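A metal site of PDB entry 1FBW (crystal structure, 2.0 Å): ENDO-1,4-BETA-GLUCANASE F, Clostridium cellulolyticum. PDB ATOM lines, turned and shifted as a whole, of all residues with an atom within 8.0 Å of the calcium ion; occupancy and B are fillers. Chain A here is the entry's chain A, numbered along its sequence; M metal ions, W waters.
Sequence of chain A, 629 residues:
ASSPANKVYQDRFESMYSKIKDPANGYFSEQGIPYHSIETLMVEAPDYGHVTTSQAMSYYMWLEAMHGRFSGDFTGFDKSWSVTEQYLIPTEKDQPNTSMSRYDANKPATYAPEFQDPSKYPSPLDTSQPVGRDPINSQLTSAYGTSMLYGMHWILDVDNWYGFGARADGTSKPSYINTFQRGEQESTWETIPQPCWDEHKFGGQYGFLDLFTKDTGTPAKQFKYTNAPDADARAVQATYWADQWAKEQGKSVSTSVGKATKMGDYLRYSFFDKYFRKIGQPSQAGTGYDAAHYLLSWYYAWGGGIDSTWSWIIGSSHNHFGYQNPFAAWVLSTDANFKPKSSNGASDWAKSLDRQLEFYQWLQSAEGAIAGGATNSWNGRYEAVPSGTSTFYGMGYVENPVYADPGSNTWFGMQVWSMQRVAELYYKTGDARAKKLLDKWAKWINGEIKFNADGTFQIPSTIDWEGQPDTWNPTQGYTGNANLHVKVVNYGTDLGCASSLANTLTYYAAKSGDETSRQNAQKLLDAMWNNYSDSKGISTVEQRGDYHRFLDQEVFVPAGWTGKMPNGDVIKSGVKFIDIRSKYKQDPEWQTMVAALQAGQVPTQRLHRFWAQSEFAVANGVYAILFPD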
ATOM      1  N   GLN A 116       7.163   4.042  31.063  1.00  0.00           N
ATOM      2  CA  GLN A 116       7.828   3.988  29.758  1.00  0.00           C
ATOM      3  C   GLN A 116       8.409   5.312  29.254  1.00  0.00           C
ATOM      4  O   GLN A 116       8.944   5.394  28.163  1.00  0.00           O
ATOM      5  CB  GLN A 116       6.902   3.355  28.716  1.00  0.00           C
ATOM      6  CG  GLN A 116       6.839   1.817  28.816  1.00  0.00           C
ATOM      7  CD  GLN A 116       6.236   1.333  30.127  1.00  0.00           C
ATOM      8  OE1 GLN A 116       5.087   1.630  30.421  1.00  0.00           O
ATOM      9  NE2 GLN A 116       7.015   0.596  30.926  1.00  0.00           N
ATOM     10  N   ASP A 117       8.265   6.366  30.049  1.00  0.00           N
ATOM     11  CA  ASP A 117       8.861   7.645  29.692  1.00  0.00           C
ATOM     12  C   ASP A 117       9.372   8.311  30.959  1.00  0.00           C
ATOM     13  O   ASP A 117       8.668   8.348  31.973  1.00  0.00           O
ATOM     14  CB  ASP A 117       7.853   8.565  29.001  1.00  0.00           C
ATOM     15  CG  ASP A 117       8.524   9.818  28.475  1.00  0.00           C
ATOM     16  OD1 ASP A 117       9.289   9.719  27.481  1.00  0.00           O
ATOM     17  OD2 ASP A 117       8.344  10.890  29.072  1.00  0.00           O
ATOM     18  N   PRO A 118      10.593   8.875  30.906  1.00  0.00           N
ATOM     19  CA  PRO A 118      11.183   9.551  32.067  1.00  0.00           C
ATOM     20  C   PRO A 118      10.337  10.672  32.681  1.00  0.00           C
ATOM     21  O   PRO A 118      10.510  10.984  33.855  1.00  0.00           O
ATOM     22  CB  PRO A 118      12.497  10.104  31.519  1.00  0.00           C
ATOM     23  CG  PRO A 118      12.829   9.151  30.416  1.00  0.00           C
ATOM     24  CD  PRO A 118      11.507   8.912  29.753  1.00  0.00           C
ATOM     25  N   GLY A 183      13.462   4.084  34.055  1.00  0.00           N
ATOM     26  CA  GLY A 183      12.910   3.225  33.018  1.00  0.00           C
ATOM     27  C   GLY A 183      13.609   3.037  31.697  1.00  0.00           C
ATOM     28  O   GLY A 183      14.649   3.630  31.417  1.00  0.00           O
ATOM     29  N   GLU A 184      12.939   2.265  30.845  1.00  0.00           N
ATOM     30  CA  GLU A 184      13.403   1.879  29.519  1.00  0.00           C
ATOM     31  C   GLU A 184      13.729   2.985  28.536  1.00  0.00           C
ATOM     32  O   GLU A 184      14.514   2.771  27.611  1.00  0.00           O
ATOM     33  CB  GLU A 184      12.408   0.901  28.880  1.00  0.00           C
ATOM     34  CG  GLU A 184      11.063   1.527  28.557  1.00  0.00           C
ATOM     35  CD  GLU A 184      10.203   0.646  27.659  1.00  0.00           C
ATOM     36  OE1 GLU A 184      10.084  -0.563  27.928  1.00  0.00           O
ATOM     37  OE2 GLU A 184       9.644   1.174  26.667  1.00  0.00           O
ATOM     38  N   GLN A 185      13.101   4.145  28.678  1.00  0.00           N
ATOM     39  CA  GLN A 185      13.419   5.230  27.758  1.00  0.00           C
ATOM     40  C   GLN A 185      14.499   6.178  28.284  1.00  0.00           C
ATOM     41  O   GLN A 185      14.838   7.151  27.623  1.00  0.00           O
ATOM     42  CB  GLN A 185      12.164   6.006  27.310  1.00  0.00           C
ATOM     43  CG  GLN A 185      11.571   5.462  26.017  1.00  0.00           C
ATOM     44  CD  GLN A 185      12.476   5.700  24.825  1.00  0.00           C
ATOM     45  OE1 GLN A 185      13.328   6.586  24.831  1.00  0.00           O
ATOM     46  NE2 GLN A 185      12.290   4.906  23.785  1.00  0.00           N
ATOM     47  N   GLU A 186      15.029   5.915  29.464  1.00  0.00           N
ATOM     48  CA  GLU A 186      16.087   6.780  29.973  1.00  0.00           C
ATOM     49  C   GLU A 186      17.452   6.260  29.528  1.00  0.00           C
ATOM     50  O   GLU A 186      18.000   5.342  30.139  1.00  0.00           O
ATOM     51  CB  GLU A 186      16.034   6.892  31.503  1.00  0.00           C
ATOM     52  CG  GLU A 186      17.015   7.922  32.057  1.00  0.00           C
ATOM     53  CD  GLU A 186      17.102   7.897  33.563  1.00  0.00           C
ATOM     54  OE1 GLU A 186      17.307   6.809  34.112  1.00  0.00           O
ATOM     55  OE2 GLU A 186      17.012   8.979  34.189  1.00  0.00           O
ATOM     56  N   SER A 187      17.979   6.799  28.430  1.00  0.00           N
ATOM     57  CA  SER A 187      19.295   6.405  27.916  1.00  0.00           C
ATOM     58  C   SER A 187      20.355   7.050  28.818  1.00  0.00           C
ATOM     59  O   SER A 187      20.024   7.810  29.720  1.00  0.00           O
ATOM     60  CB  SER A 187      19.480   6.915  26.490  1.00  0.00           C
ATOM     61  OG  SER A 187      19.511   8.342  26.444  1.00  0.00           O
ATOM     62  N   THR A 188      21.627   6.766  28.553  1.00  0.00           N
ATOM     63  CA  THR A 188      22.748   7.346  29.299  1.00  0.00           C
ATOM     64  C   THR A 188      22.760   8.865  29.190  1.00  0.00           C
ATOM     65  O   THR A 188      23.371   9.539  30.026  1.00  0.00           O
ATOM     66  CB  THR A 188      24.090   6.936  28.707  1.00  0.00           C
ATOM     67  OG1 THR A 188      24.045   5.584  28.273  1.00  0.00           O
ATOM     68  CG2 THR A 188      25.155   7.062  29.727  1.00  0.00           C
ATOM     69  N   TRP A 189      22.167   9.385  28.120  1.00  0.00           N
ATOM     70  CA  TRP A 189      22.117  10.825  27.868  1.00  0.00           C
ATOM     71  C   TRP A 189      21.017  11.532  28.637  1.00  0.00           C
ATOM     72  O   TRP A 189      20.991  12.752  28.714  1.00  0.00           O
ATOM     73  CB  TRP A 189      21.859  11.073  26.386  1.00  0.00           C
ATOM     74  CG  TRP A 189      22.865  10.426  25.512  1.00  0.00           C
ATOM     75  CD1 TRP A 189      22.761   9.229  24.861  1.00  0.00           C
ATOM     76  CD2 TRP A 189      24.146  10.950  25.182  1.00  0.00           C
ATOM     77  NE1 TRP A 189      23.908   8.980  24.136  1.00  0.00           N
ATOM     78  CE2 TRP A 189      24.774  10.015  24.322  1.00  0.00           C
ATOM     79  CE3 TRP A 189      24.838  12.117  25.532  1.00  0.00           C
ATOM     80  CZ2 TRP A 189      26.054  10.226  23.804  1.00  0.00           C
ATOM     81  CZ3 TRP A 189      26.105  12.325  25.021  1.00  0.00           C
ATOM     82  CH2 TRP A 189      26.705  11.371  24.160  1.00  0.00           C
ATOM     83  N   GLU A 190      20.131  10.754  29.240  1.00  0.00           N
ATOM     84  CA  GLU A 190      18.971  11.305  29.921  1.00  0.00           C
ATOM     85  C   GLU A 190      18.883  11.188  31.417  1.00  0.00           C
ATOM     86  O   GLU A 190      17.833  11.494  32.017  1.00  0.00           O
ATOM     87  CB  GLU A 190      17.722  10.696  29.287  1.00  0.00           C
ATOM     88  CG  GLU A 190      17.498  11.203  27.879  1.00  0.00           C
ATOM     89  CD  GLU A 190      16.552  10.322  27.137  1.00  0.00           C
ATOM     90  OE1 GLU A 190      17.007   9.271  26.662  1.00  0.00           O
ATOM     91  OE2 GLU A 190      15.351  10.653  27.071  1.00  0.00           O
ATOM     92  N   ALA A 404      15.071   0.528  25.731  1.00  0.00           N
ATOM     93  CA  ALA A 404      14.599   0.720  24.359  1.00  0.00           C
ATOM     94  C   ALA A 404      15.379   1.836  23.668  1.00  0.00           C
ATOM     95  O   ALA A 404      15.228   2.031  22.461  1.00  0.00           O
ATOM     96  CB  ALA A 404      13.106   1.070  24.390  1.00  0.00           C
ATOM     97  N   ASP A 405      16.249   2.519  24.407  1.00  0.00           N
ATOM     98  CA  ASP A 405      17.007   3.634  23.837  1.00  0.00           C
ATOM     99  C   ASP A 405      18.505   3.548  24.136  1.00  0.00           C
ATOM    100  O   ASP A 405      18.978   4.144  25.089  1.00  0.00           O
ATOM    101  CB  ASP A 405      16.458   4.945  24.414  1.00  0.00           C
ATOM    102  CG  ASP A 405      17.040   6.189  23.760  1.00  0.00           C
ATOM    103  OD1 ASP A 405      17.925   6.095  22.888  1.00  0.00           O
ATOM    104  OD2 ASP A 405      16.575   7.298  24.144  1.00  0.00           O
ATOM    105  N   PRO A 406      19.260   2.806  23.308  1.00  0.00           N
ATOM    106  CA  PRO A 406      18.774   2.038  22.167  1.00  0.00           C
ATOM    107  C   PRO A 406      18.345   0.662  22.678  1.00  0.00           C
ATOM    108  O   PRO A 406      18.528   0.357  23.862  1.00  0.00           O
ATOM    109  CB  PRO A 406      20.015   1.952  21.290  1.00  0.00           C
ATOM    110  CG  PRO A 406      21.102   1.798  22.292  1.00  0.00           C
ATOM    111  CD  PRO A 406      20.730   2.789  23.374  1.00  0.00           C
ATOM    112  N   ARG A 549      23.936  14.293  20.909  1.00  0.00           N
ATOM    113  CA  ARG A 549      23.121  14.346  22.128  1.00  0.00           C
ATOM    114  C   ARG A 549      23.773  15.103  23.305  1.00  0.00           C
ATOM    115  O   ARG A 549      23.092  15.451  24.269  1.00  0.00           O
ATOM    116  CB  ARG A 549      22.680  12.939  22.547  1.00  0.00           C
ATOM    117  CG  ARG A 549      21.764  12.279  21.512  1.00  0.00           C
ATOM    118  CD  ARG A 549      21.415  10.860  21.910  1.00  0.00           C
ATOM    119  NE  ARG A 549      20.244  10.821  22.778  1.00  0.00           N
ATOM    120  CZ  ARG A 549      19.524   9.722  23.002  1.00  0.00           C
ATOM    121  NH1 ARG A 549      19.881   8.582  22.434  1.00  0.00           N
ATOM    122  NH2 ARG A 549      18.406   9.794  23.724  1.00  0.00           N
ATOM    123  N   GLN A 553      20.368  16.865  23.723  1.00  0.00           N
ATOM    124  CA  GLN A 553      19.455  16.018  24.480  1.00  0.00           C
ATOM    125  C   GLN A 553      18.921  16.750  25.698  1.00  0.00           C
ATOM    126  O   GLN A 553      19.701  17.140  26.566  1.00  0.00           O
ATOM    127  CB  GLN A 553      20.125  14.716  24.951  1.00  0.00           C
ATOM    128  CG  GLN A 553      19.195  13.850  25.814  1.00  0.00           C
ATOM    129  CD  GLN A 553      18.049  13.289  25.005  1.00  0.00           C
ATOM    130  OE1 GLN A 553      18.260  12.523  24.067  1.00  0.00           O
ATOM    131  NE2 GLN A 553      16.829  13.680  25.350  1.00  0.00           N
ATOM    132  N   GLU A 554      17.615  16.945  25.764  1.00  0.00           N
ATOM    133  CA  GLU A 554      17.004  17.587  26.923  1.00  0.00           C
ATOM    134  C   GLU A 554      16.874  16.548  28.029  1.00  0.00           C
ATOM    135  O   GLU A 554      16.550  15.390  27.781  1.00  0.00           O
ATOM    136  CB  GLU A 554      15.619  18.138  26.584  1.00  0.00           C
ATOM    137  CG  GLU A 554      15.063  19.010  27.712  1.00  0.00           C
ATOM    138  CD  GLU A 554      13.713  19.622  27.388  1.00  0.00           C
ATOM    139  OE1 GLU A 554      13.626  20.349  26.375  1.00  0.00           O
ATOM    140  OE2 GLU A 554      12.754  19.383  28.170  1.00  0.00           O
HETATM  141 CA    CA M   1      14.834   8.457  25.602  1.00  0.00          CA
HETATM  142  O   HOH W   1      12.579   9.476  26.028  1.00  0.00           O
HETATM  143  O   HOH W   2      15.049   9.971  23.691  1.00  0.00           O
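OE1 of Glu 190 lies close to NH2 of Arg 549, at 3.3 Å.
NH1 of Arg 549 is in salt-bridge range of OD1 of Asp 405 (3.2 Å).
The side-chain hydroxyl (OG) of Ser 187 lies close to the side-chain carboxylate (OE1) of Glu 190 (2.7 Å).
Of the 17 residues printed, 3 come within 4 Å of the calcium ion.
The calcium ion is bound by O of Gln 185 (2.4 Å), water W2 (2.4 Å), water W1 (2.5 Å), OE1 of Gln 185 (2.5 Å), OD2 of Asp 405 (2.5 Å), OE1 of Glu 190 (2.6 Å) and OE2 of Glu 190 (2.7 Å).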
